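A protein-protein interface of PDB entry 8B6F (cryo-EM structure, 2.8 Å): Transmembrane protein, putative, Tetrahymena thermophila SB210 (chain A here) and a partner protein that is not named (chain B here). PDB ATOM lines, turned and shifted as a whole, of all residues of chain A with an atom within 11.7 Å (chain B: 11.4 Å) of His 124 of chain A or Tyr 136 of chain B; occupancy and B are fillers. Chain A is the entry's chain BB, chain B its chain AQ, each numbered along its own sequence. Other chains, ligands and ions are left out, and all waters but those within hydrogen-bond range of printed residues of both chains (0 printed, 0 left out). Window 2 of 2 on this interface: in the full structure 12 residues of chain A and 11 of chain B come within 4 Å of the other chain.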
ATOM      1  N   GLY A 118     -12.168  27.755   6.631  1.00  0.00           N
ATOM      2  CA  GLY A 118     -12.352  27.731   8.065  1.00  0.00           C
ATOM      3  C   GLY A 118     -11.870  26.485   8.764  1.00  0.00           C
ATOM      4  O   GLY A 118     -11.928  26.424   9.993  1.00  0.00           O
ATOM      5  N   LEU A 119     -11.401  25.481   8.020  1.00  0.00           N
ATOM      6  CA  LEU A 119     -10.923  24.234   8.606  1.00  0.00           C
ATOM      7  C   LEU A 119      -9.434  24.007   8.379  1.00  0.00           C
ATOM      8  O   LEU A 119      -8.935  22.915   8.677  1.00  0.00           O
ATOM      9  CB  LEU A 119     -11.727  23.053   8.057  1.00  0.00           C
ATOM     10  CG  LEU A 119     -13.170  22.962   8.567  1.00  0.00           C
ATOM     11  CD1 LEU A 119     -13.960  21.940   7.779  1.00  0.00           C
ATOM     12  CD2 LEU A 119     -13.206  22.619  10.047  1.00  0.00           C
ATOM     13  N   MET A 120      -8.711  24.994   7.855  1.00  0.00           N
ATOM     14  CA  MET A 120      -7.257  24.928   7.825  1.00  0.00           C
ATOM     15  C   MET A 120      -6.716  25.292   9.199  1.00  0.00           C
ATOM     16  O   MET A 120      -7.054  26.344   9.750  1.00  0.00           O
ATOM     17  CB  MET A 120      -6.688  25.874   6.769  1.00  0.00           C
ATOM     18  CG  MET A 120      -6.837  25.387   5.340  1.00  0.00           C
ATOM     19  SD  MET A 120      -6.024  23.806   5.023  1.00  0.00           S
ATOM     20  CE  MET A 120      -4.329  24.180   5.453  1.00  0.00           C
ATOM     21  N   ASN A 121      -5.879  24.425   9.750  1.00  0.00           N
ATOM     22  CA  ASN A 121      -5.408  24.568  11.118  1.00  0.00           C
ATOM     23  C   ASN A 121      -4.043  25.238  11.144  1.00  0.00           C
ATOM     24  O   ASN A 121      -3.167  24.926  10.332  1.00  0.00           O
ATOM     25  CB  ASN A 121      -5.325  23.204  11.807  1.00  0.00           C
ATOM     26  CG  ASN A 121      -6.659  22.493  11.850  1.00  0.00           C
ATOM     27  OD1 ASN A 121      -7.705  23.120  12.002  1.00  0.00           O
ATOM     28  ND2 ASN A 121      -6.630  21.174  11.709  1.00  0.00           N
ATOM     29  N   GLU A 122      -3.882  26.172  12.056  1.00  0.00           N
ATOM     30  CA  GLU A 122      -2.580  26.693  12.424  1.00  0.00           C
ATOM     31  C   GLU A 122      -1.992  25.838  13.536  1.00  0.00           C
ATOM     32  O   GLU A 122      -2.719  25.100  14.208  1.00  0.00           O
ATOM     33  CB  GLU A 122      -2.706  28.146  12.874  1.00  0.00           C
ATOM     34  CG  GLU A 122      -3.094  29.094  11.753  1.00  0.00           C
ATOM     35  CD  GLU A 122      -3.148  30.537  12.208  1.00  0.00           C
ATOM     36  OE1 GLU A 122      -2.882  30.793  13.400  1.00  0.00           O
ATOM     37  OE2 GLU A 122      -3.456  31.415  11.376  1.00  0.00           O
ATOM     38  N   PRO A 123      -0.681  25.891  13.755  1.00  0.00           N
ATOM     39  CA  PRO A 123      -0.088  25.046  14.797  1.00  0.00           C
ATOM     40  C   PRO A 123      -0.801  25.235  16.127  1.00  0.00           C
ATOM     41  O   PRO A 123      -1.060  26.359  16.563  1.00  0.00           O
ATOM     42  CB  PRO A 123       1.371  25.519  14.853  1.00  0.00           C
ATOM     43  CG  PRO A 123       1.413  26.801  14.078  1.00  0.00           C
ATOM     44  CD  PRO A 123       0.338  26.689  13.058  1.00  0.00           C
ATOM     45  N   HIS A 124      -1.129  24.121  16.771  1.00  0.00           N
ATOM     46  CA  HIS A 124      -1.928  24.140  17.989  1.00  0.00           C
ATOM     47  C   HIS A 124      -1.657  22.856  18.763  1.00  0.00           C
ATOM     48  O   HIS A 124      -0.934  21.968  18.304  1.00  0.00           O
ATOM     49  CB  HIS A 124      -3.419  24.290  17.673  1.00  0.00           C
ATOM     50  CG  HIS A 124      -3.997  23.128  16.928  1.00  0.00           C
ATOM     51  ND1 HIS A 124      -4.239  21.909  17.524  1.00  0.00           N
ATOM     52  CD2 HIS A 124      -4.377  22.995  15.636  1.00  0.00           C
ATOM     53  CE1 HIS A 124      -4.743  21.076  16.632  1.00  0.00           C
ATOM     54  NE2 HIS A 124      -4.837  21.711  15.478  1.00  0.00           N
ATOM     55  N   GLY A 125      -2.253  22.765  19.944  1.00  0.00           N
ATOM     56  CA  GLY A 125      -2.104  21.619  20.812  1.00  0.00           C
ATOM     57  C   GLY A 125      -1.072  21.858  21.900  1.00  0.00           C
ATOM     58  O   GLY A 125      -0.218  22.743  21.814  1.00  0.00           O
ATOM     59  N   TYR A 126      -1.159  21.044  22.947  1.00  0.00           N
ATOM     60  CA  TYR A 126      -0.237  21.108  24.072  1.00  0.00           C
ATOM     61  C   TYR A 126       0.855  20.070  23.872  1.00  0.00           C
ATOM     62  O   TYR A 126       0.566  18.904  23.587  1.00  0.00           O
ATOM     63  CB  TYR A 126      -0.966  20.871  25.395  1.00  0.00           C
ATOM     64  CG  TYR A 126      -2.053  21.882  25.668  1.00  0.00           C
ATOM     65  CD1 TYR A 126      -1.739  23.188  26.017  1.00  0.00           C
ATOM     66  CD2 TYR A 126      -3.391  21.530  25.575  1.00  0.00           C
ATOM     67  CE1 TYR A 126      -2.728  24.116  26.265  1.00  0.00           C
ATOM     68  CE2 TYR A 126      -4.387  22.450  25.821  1.00  0.00           C
ATOM     69  CZ  TYR A 126      -4.049  23.741  26.165  1.00  0.00           C
ATOM     70  OH  TYR A 126      -5.040  24.660  26.413  1.00  0.00           O
ATOM     71  N   LEU A 127       2.110  20.497  24.023  1.00  0.00           N
ATOM     72  CA  LEU A 127       3.227  19.603  23.749  1.00  0.00           C
ATOM     73  C   LEU A 127       3.201  18.385  24.662  1.00  0.00           C
ATOM     74  O   LEU A 127       3.430  17.257  24.213  1.00  0.00           O
ATOM     75  CB  LEU A 127       4.546  20.362  23.903  1.00  0.00           C
ATOM     76  CG  LEU A 127       5.820  19.611  23.514  1.00  0.00           C
ATOM     77  CD1 LEU A 127       5.808  19.241  22.038  1.00  0.00           C
ATOM     78  CD2 LEU A 127       7.048  20.440  23.849  1.00  0.00           C
ATOM     79  N   THR A 128       2.923  18.593  25.945  1.00  0.00           N
ATOM     80  CA  THR A 128       2.880  17.529  26.937  1.00  0.00           C
ATOM     81  C   THR A 128       1.619  17.680  27.776  1.00  0.00           C
ATOM     82  O   THR A 128       0.815  18.592  27.573  1.00  0.00           O
ATOM     83  CB  THR A 128       4.116  17.554  27.839  1.00  0.00           C
ATOM     84  OG1 THR A 128       4.195  18.827  28.484  1.00  0.00           O
ATOM     85  CG2 THR A 128       5.380  17.323  27.024  1.00  0.00           C
ATOM     86  N   ASP A 130       1.636  18.354  30.955  1.00  0.00           N
ATOM     87  CA  ASP A 130       1.845  19.290  32.051  1.00  0.00           C
ATOM     88  C   ASP A 130       1.040  20.566  31.833  1.00  0.00           C
ATOM     89  O   ASP A 130       0.984  21.105  30.725  1.00  0.00           O
ATOM     90  CB  ASP A 130       3.328  19.629  32.189  1.00  0.00           C
ATOM     91  CG  ASP A 130       4.148  18.458  32.685  1.00  0.00           C
ATOM     92  OD1 ASP A 130       3.633  17.323  32.664  1.00  0.00           O
ATOM     93  OD2 ASP A 130       5.301  18.676  33.111  1.00  0.00           O
ATOM     94  N   ASP A 131       0.428  21.052  32.904  1.00  0.00           N
ATOM     95  CA  ASP A 131      -0.376  22.266  32.819  1.00  0.00           C
ATOM     96  C   ASP A 131       0.537  23.484  32.709  1.00  0.00           C
ATOM     97  O   ASP A 131       1.417  23.668  33.557  1.00  0.00           O
ATOM     98  CB  ASP A 131      -1.273  22.382  34.049  1.00  0.00           C
ATOM     99  CG  ASP A 131      -2.271  23.520  33.944  1.00  0.00           C
ATOM    100  OD1 ASP A 131      -1.998  24.497  33.218  1.00  0.00           O
ATOM    101  OD2 ASP A 131      -3.331  23.440  34.597  1.00  0.00           O
ATOM    102  N   PRO A 132       0.369  24.333  31.689  1.00  0.00           N
ATOM    103  CA  PRO A 132       1.226  25.526  31.602  1.00  0.00           C
ATOM    104  C   PRO A 132       1.156  26.409  32.833  1.00  0.00           C
ATOM    105  O   PRO A 132       2.172  26.990  33.232  1.00  0.00           O
ATOM    106  CB  PRO A 132       0.693  26.249  30.358  1.00  0.00           C
ATOM    107  CG  PRO A 132       0.041  25.195  29.552  1.00  0.00           C
ATOM    108  CD  PRO A 132      -0.536  24.222  30.532  1.00  0.00           C
ATOM    109  N   MET A 133      -0.017  26.534  33.442  1.00  0.00           N
ATOM    110  CA  MET A 133      -0.212  27.342  34.642  1.00  0.00           C
ATOM    111  C   MET A 133      -0.533  26.383  35.785  1.00  0.00           C
ATOM    112  O   MET A 133      -1.697  26.129  36.096  1.00  0.00           O
ATOM    113  CB  MET A 133      -1.323  28.370  34.439  1.00  0.00           C
ATOM    114  CG  MET A 133      -1.153  29.207  33.182  1.00  0.00           C
ATOM    115  SD  MET A 133      -2.338  30.558  33.064  1.00  0.00           S
ATOM    116  CE  MET A 133      -1.794  31.601  34.413  1.00  0.00           C
ATOM    117  N   PHE B 123     -13.078  13.238  14.837  1.00  0.00           N
ATOM    118  CA  PHE B 123     -13.071  13.582  16.251  1.00  0.00           C
ATOM    119  C   PHE B 123     -14.457  14.021  16.704  1.00  0.00           C
ATOM    120  O   PHE B 123     -15.128  14.809  16.032  1.00  0.00           O
ATOM    121  CB  PHE B 123     -12.052  14.686  16.521  1.00  0.00           C
ATOM    122  CG  PHE B 123     -10.638  14.284  16.226  1.00  0.00           C
ATOM    123  CD1 PHE B 123      -9.876  13.637  17.182  1.00  0.00           C
ATOM    124  CD2 PHE B 123     -10.071  14.552  14.993  1.00  0.00           C
ATOM    125  CE1 PHE B 123      -8.574  13.265  16.916  1.00  0.00           C
ATOM    126  CE2 PHE B 123      -8.770  14.181  14.719  1.00  0.00           C
ATOM    127  CZ  PHE B 123      -8.020  13.537  15.683  1.00  0.00           C
ATOM    128  N   LEU B 127     -14.113  15.293  22.300  1.00  0.00           N
ATOM    129  CA  LEU B 127     -12.713  15.663  22.120  1.00  0.00           C
ATOM    130  C   LEU B 127     -12.573  17.131  21.739  1.00  0.00           C
ATOM    131  O   LEU B 127     -11.647  17.809  22.196  1.00  0.00           O
ATOM    132  CB  LEU B 127     -12.068  14.770  21.061  1.00  0.00           C
ATOM    133  CG  LEU B 127     -11.920  13.299  21.451  1.00  0.00           C
ATOM    134  CD1 LEU B 127     -11.433  12.483  20.272  1.00  0.00           C
ATOM    135  CD2 LEU B 127     -10.972  13.143  22.629  1.00  0.00           C
ATOM    136  N   LEU B 128     -13.477  17.637  20.898  1.00  0.00           N
ATOM    137  CA  LEU B 128     -13.398  19.034  20.487  1.00  0.00           C
ATOM    138  C   LEU B 128     -13.553  19.969  21.679  1.00  0.00           C
ATOM    139  O   LEU B 128     -12.830  20.963  21.796  1.00  0.00           O
ATOM    140  CB  LEU B 128     -14.459  19.329  19.425  1.00  0.00           C
ATOM    141  CG  LEU B 128     -14.364  18.516  18.129  1.00  0.00           C
ATOM    142  CD1 LEU B 128     -15.467  18.914  17.166  1.00  0.00           C
ATOM    143  CD2 LEU B 128     -13.006  18.672  17.469  1.00  0.00           C
ATOM    144  N   LYS B 129     -14.493  19.665  22.577  1.00  0.00           N
ATOM    145  CA  LYS B 129     -14.681  20.498  23.761  1.00  0.00           C
ATOM    146  C   LYS B 129     -13.533  20.333  24.747  1.00  0.00           C
ATOM    147  O   LYS B 129     -13.145  21.294  25.420  1.00  0.00           O
ATOM    148  CB  LYS B 129     -16.005  20.156  24.445  1.00  0.00           C
ATOM    149  CG  LYS B 129     -17.240  20.551  23.655  1.00  0.00           C
ATOM    150  CD  LYS B 129     -18.507  20.420  24.490  1.00  0.00           C
ATOM    151  CE  LYS B 129     -18.677  19.022  25.067  1.00  0.00           C
ATOM    152  NZ  LYS B 129     -18.599  17.966  24.023  1.00  0.00           N
ATOM    153  N   PHE B 130     -12.987  19.126  24.855  1.00  0.00           N
ATOM    154  CA  PHE B 130     -11.984  18.833  25.870  1.00  0.00           C
ATOM    155  C   PHE B 130     -10.836  19.828  25.806  1.00  0.00           C
ATOM    156  O   PHE B 130     -10.183  19.978  24.771  1.00  0.00           O
ATOM    157  CB  PHE B 130     -11.466  17.406  25.686  1.00  0.00           C
ATOM    158  CG  PHE B 130     -10.513  16.973  26.756  1.00  0.00           C
ATOM    159  CD1 PHE B 130     -10.959  16.748  28.046  1.00  0.00           C
ATOM    160  CD2 PHE B 130      -9.176  16.777  26.472  1.00  0.00           C
ATOM    161  CE1 PHE B 130     -10.085  16.346  29.035  1.00  0.00           C
ATOM    162  CE2 PHE B 130      -8.299  16.374  27.455  1.00  0.00           C
ATOM    163  CZ  PHE B 130      -8.753  16.158  28.738  1.00  0.00           C
ATOM    164  N   ASP B 131     -10.598  20.511  26.923  1.00  0.00           N
ATOM    165  CA  ASP B 131      -9.530  21.494  27.031  1.00  0.00           C
ATOM    166  C   ASP B 131      -9.223  21.741  28.504  1.00  0.00           C
ATOM    167  O   ASP B 131      -9.660  22.754  29.065  1.00  0.00           O
ATOM    168  CB  ASP B 131      -9.928  22.795  26.337  1.00  0.00           C
ATOM    169  CG  ASP B 131      -8.810  23.815  26.329  1.00  0.00           C
ATOM    170  OD1 ASP B 131      -7.659  23.440  26.630  1.00  0.00           O
ATOM    171  OD2 ASP B 131      -9.083  24.994  26.027  1.00  0.00           O
ATOM    172  N   PRO B 132      -8.484  20.847  29.163  1.00  0.00           N
ATOM    173  CA  PRO B 132      -8.261  21.019  30.607  1.00  0.00           C
ATOM    174  C   PRO B 132      -7.546  22.306  30.959  1.00  0.00           C
ATOM    175  O   PRO B 132      -7.783  22.862  32.038  1.00  0.00           O
ATOM    176  CB  PRO B 132      -7.428  19.785  30.982  1.00  0.00           C
ATOM    177  CG  PRO B 132      -6.792  19.353  29.721  1.00  0.00           C
ATOM    178  CD  PRO B 132      -7.730  19.709  28.614  1.00  0.00           C
ATOM    179  N   PHE B 133      -6.673  22.795  30.089  1.00  0.00           N
ATOM    180  CA  PHE B 133      -5.988  24.056  30.313  1.00  0.00           C
ATOM    181  C   PHE B 133      -6.755  25.178  29.622  1.00  0.00           C
ATOM    182  O   PHE B 133      -7.593  24.944  28.749  1.00  0.00           O
ATOM    183  CB  PHE B 133      -4.548  23.977  29.807  1.00  0.00           C
ATOM    184  CG  PHE B 133      -3.858  22.685  30.155  1.00  0.00           C
ATOM    185  CD1 PHE B 133      -4.110  22.048  31.359  1.00  0.00           C
ATOM    186  CD2 PHE B 133      -2.972  22.099  29.269  1.00  0.00           C
ATOM    187  CE1 PHE B 133      -3.483  20.856  31.673  1.00  0.00           C
ATOM    188  CE2 PHE B 133      -2.344  20.909  29.577  1.00  0.00           C
ATOM    189  CZ  PHE B 133      -2.599  20.286  30.781  1.00  0.00           C
ATOM    190  N   GLY B 134      -6.466  26.409  30.025  1.00  0.00           N
ATOM    191  CA  GLY B 134      -7.303  27.525  29.637  1.00  0.00           C
ATOM    192  C   GLY B 134      -6.859  28.290  28.408  1.00  0.00           C
ATOM    193  O   GLY B 134      -7.298  29.425  28.201  1.00  0.00           O
ATOM    194  N   PHE B 135      -6.000  27.698  27.578  1.00  0.00           N
ATOM    195  CA  PHE B 135      -5.483  28.434  26.429  1.00  0.00           C
ATOM    196  C   PHE B 135      -6.564  28.645  25.374  1.00  0.00           C
ATOM    197  O   PHE B 135      -6.726  29.756  24.856  1.00  0.00           O
ATOM    198  CB  PHE B 135      -4.283  27.707  25.828  1.00  0.00           C
ATOM    199  CG  PHE B 135      -3.578  28.501  24.769  1.00  0.00           C
ATOM    200  CD1 PHE B 135      -2.623  29.441  25.116  1.00  0.00           C
ATOM    201  CD2 PHE B 135      -3.878  28.321  23.431  1.00  0.00           C
ATOM    202  CE1 PHE B 135      -1.974  30.180  24.150  1.00  0.00           C
ATOM    203  CE2 PHE B 135      -3.234  29.057  22.457  1.00  0.00           C
ATOM    204  CZ  PHE B 135      -2.281  29.988  22.817  1.00  0.00           C
ATOM    205  N   TYR B 136      -7.310  27.595  25.039  1.00  0.00           N
ATOM    206  CA  TYR B 136      -8.330  27.664  23.997  1.00  0.00           C
ATOM    207  C   TYR B 136      -9.722  27.908  24.564  1.00  0.00           C
ATOM    208  O   TYR B 136     -10.455  28.764  24.062  1.00  0.00           O
ATOM    209  CB  TYR B 136      -8.319  26.373  23.169  1.00  0.00           C
ATOM    210  CG  TYR B 136      -6.961  26.056  22.595  1.00  0.00           C
ATOM    211  CD1 TYR B 136      -6.478  26.740  21.489  1.00  0.00           C
ATOM    212  CD2 TYR B 136      -6.153  25.086  23.172  1.00  0.00           C
ATOM    213  CE1 TYR B 136      -5.234  26.461  20.966  1.00  0.00           C
ATOM    214  CE2 TYR B 136      -4.908  24.801  22.657  1.00  0.00           C
ATOM    215  CZ  TYR B 136      -4.454  25.495  21.556  1.00  0.00           C
ATOM    216  OH  TYR B 136      -3.214  25.214  21.042  1.00  0.00           O
ATOM    217  N   SER B 137     -10.101  27.169  25.605  1.00  0.00           N
ATOM    218  CA  SER B 137     -11.365  27.377  26.293  1.00  0.00           C
ATOM    219  C   SER B 137     -11.082  27.944  27.675  1.00  0.00           C
ATOM    220  O   SER B 137     -10.351  27.308  28.449  1.00  0.00           O
ATOM    221  CB  SER B 137     -12.140  26.066  26.400  1.00  0.00           C
ATOM    222  OG  SER B 137     -13.414  26.271  26.984  1.00  0.00           O
ATOM    223  N   PRO B 138     -11.625  29.107  28.040  1.00  0.00           N
ATOM    224  CA  PRO B 138     -11.210  29.746  29.295  1.00  0.00           C
ATOM    225  C   PRO B 138     -11.421  28.834  30.496  1.00  0.00           C
ATOM    226  O   PRO B 138     -12.431  28.137  30.604  1.00  0.00           O
ATOM    227  CB  PRO B 138     -12.096  30.997  29.369  1.00  0.00           C
ATOM    228  CG  PRO B 138     -13.247  30.710  28.477  1.00  0.00           C
ATOM    229  CD  PRO B 138     -12.714  29.848  27.381  1.00  0.00           C
ATOM    230  N   LYS B 139     -10.452  28.857  31.407  1.00  0.00           N
ATOM    231  CA  LYS B 139     -10.430  27.987  32.575  1.00  0.00           C
ATOM    232  C   LYS B 139     -10.614  28.832  33.828  1.00  0.00           C
ATOM    233  O   LYS B 139      -9.832  29.754  34.079  1.00  0.00           O
ATOM    234  CB  LYS B 139      -9.114  27.210  32.638  1.00  0.00           C
ATOM    235  CG  LYS B 139      -9.001  26.231  33.797  1.00  0.00           C
ATOM    236  CD  LYS B 139      -9.957  25.066  33.631  1.00  0.00           C
ATOM    237  CE  LYS B 139      -9.765  24.031  34.727  1.00  0.00           C
ATOM    238  NZ  LYS B 139      -8.397  23.439  34.714  1.00  0.00           N
ATOM    239  N   LEU B 140     -11.637  28.509  34.613  1.00  0.00           N
ATOM    240  CA  LEU B 140     -11.888  29.225  35.855  1.00  0.00           C
ATOM    241  C   LEU B 140     -10.775  28.964  36.861  1.00  0.00           C
ATOM    242  O   LEU B 140     -10.225  27.863  36.928  1.00  0.00           O
ATOM    243  CB  LEU B 140     -13.227  28.792  36.448  1.00  0.00           C
ATOM    244  CG  LEU B 140     -14.484  29.240  35.709  1.00  0.00           C
ATOM    245  CD1 LEU B 140     -15.679  28.443  36.185  1.00  0.00           C
ATOM    246  CD2 LEU B 140     -14.719  30.722  35.919  1.00  0.00           C
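N of Met 133 of chain A lies within hydrogen-bond range of OD1 of Asp 131 of chain A, 2.9 Å away.
The side-chain carboxylate of Asp 131 of chain B sits close to the backbone NH of Tyr 136 of chain B.
The side-chain carboxylate (OD1) of Asp 131 of chain B lies close to the backbone carbonyl oxygen (O) of Phe 133 of chain B (2.6 Å).
The backbone NH of Ser 137 of chain B lies within hydrogen-bond range of the side-chain carboxylate of Asp 131 of chain B.
Printed residues of chain A that touch a printed residue of chain B: His 124, Gly 125, Tyr 126, Asp 130, Asp 131 and Pro 132.
Among the printed residues, 9 pairs touch across the chains.
Among the printed residues, no Asp or Glu carboxylate lies within 4 Å of a Lys or Arg side-chain nitrogen of the other chain.
Among the printed residues, pairs that only touch across the chains: His 124 of chain A with Tyr 136 of chain B, Tyr 126 of chain A with Tyr 136 of chain B, Asp 130 of chain A with Phe 133 of chain B, Asp 131 of chain A with Phe 133 of chain B and Pro 132 of chain A with Phe 133 of chain B.
No residue of chain B comes within 4 Å of Pro 123 of chain A.
Of chain B, only Tyr 136 comes within 4 Å of His 124 of chain A.
Of the printed residues of chain B, Gly 125 of chain A touches Tyr 136.
Of the printed residues of chain B, Asp 130 of chain A touches Phe 133.
Of the printed residues of chain B, Asp 131 of chain A touches Phe 133.
Of the printed residues of chain B, Pro 132 of chain A touches Phe 133 (3.5 Å).
Of the printed residues of chain A, Phe 133 of chain B touches Tyr 126 (3.5 Å), Asp 130 (3.5 Å), Asp 131 (3.5 Å) and Pro 132 (3.5 Å).
No residue of chain A comes within 4 Å of Gly 134 of chain B.
Printed residues of chain A within 4 Å of Phe 135 of chain B: Tyr 126 (3.2 Å).
Of chain A, only His 124 (3.5 Å), Gly 125 (2.9 Å) and Tyr 126 (3.5 Å) come within 4 Å of Tyr 136 of chain B.
No residue of chain A comes within 4 Å of Ser 137 of chain B.
The nearest printed residue of chain B that does not touch Asp 130 of chain A is Pro 132 of chain B (8.0 Å).
The side-chain hydroxyl of Tyr 126 of chain A is in hydrogen-bond range of the side-chain carboxylate of Asp 131 of chain B (2.9 Å).
The side-chain hydroxyl (OH) of Tyr 126 of chain A lies close to the backbone NH (N) of Phe 135 of chain B, at 3.4 Å.
The side-chain hydroxyl (OH) of Tyr 136 of chain B sits at hydrogen-bond distance from the backbone NH (N) of Gly 125 of chain A (2.9 Å).
The side-chain hydroxyl of Tyr 126 of chain A sits at hydrogen-bond distance from the backbone carbonyl oxygen of Phe 133 of chain B.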
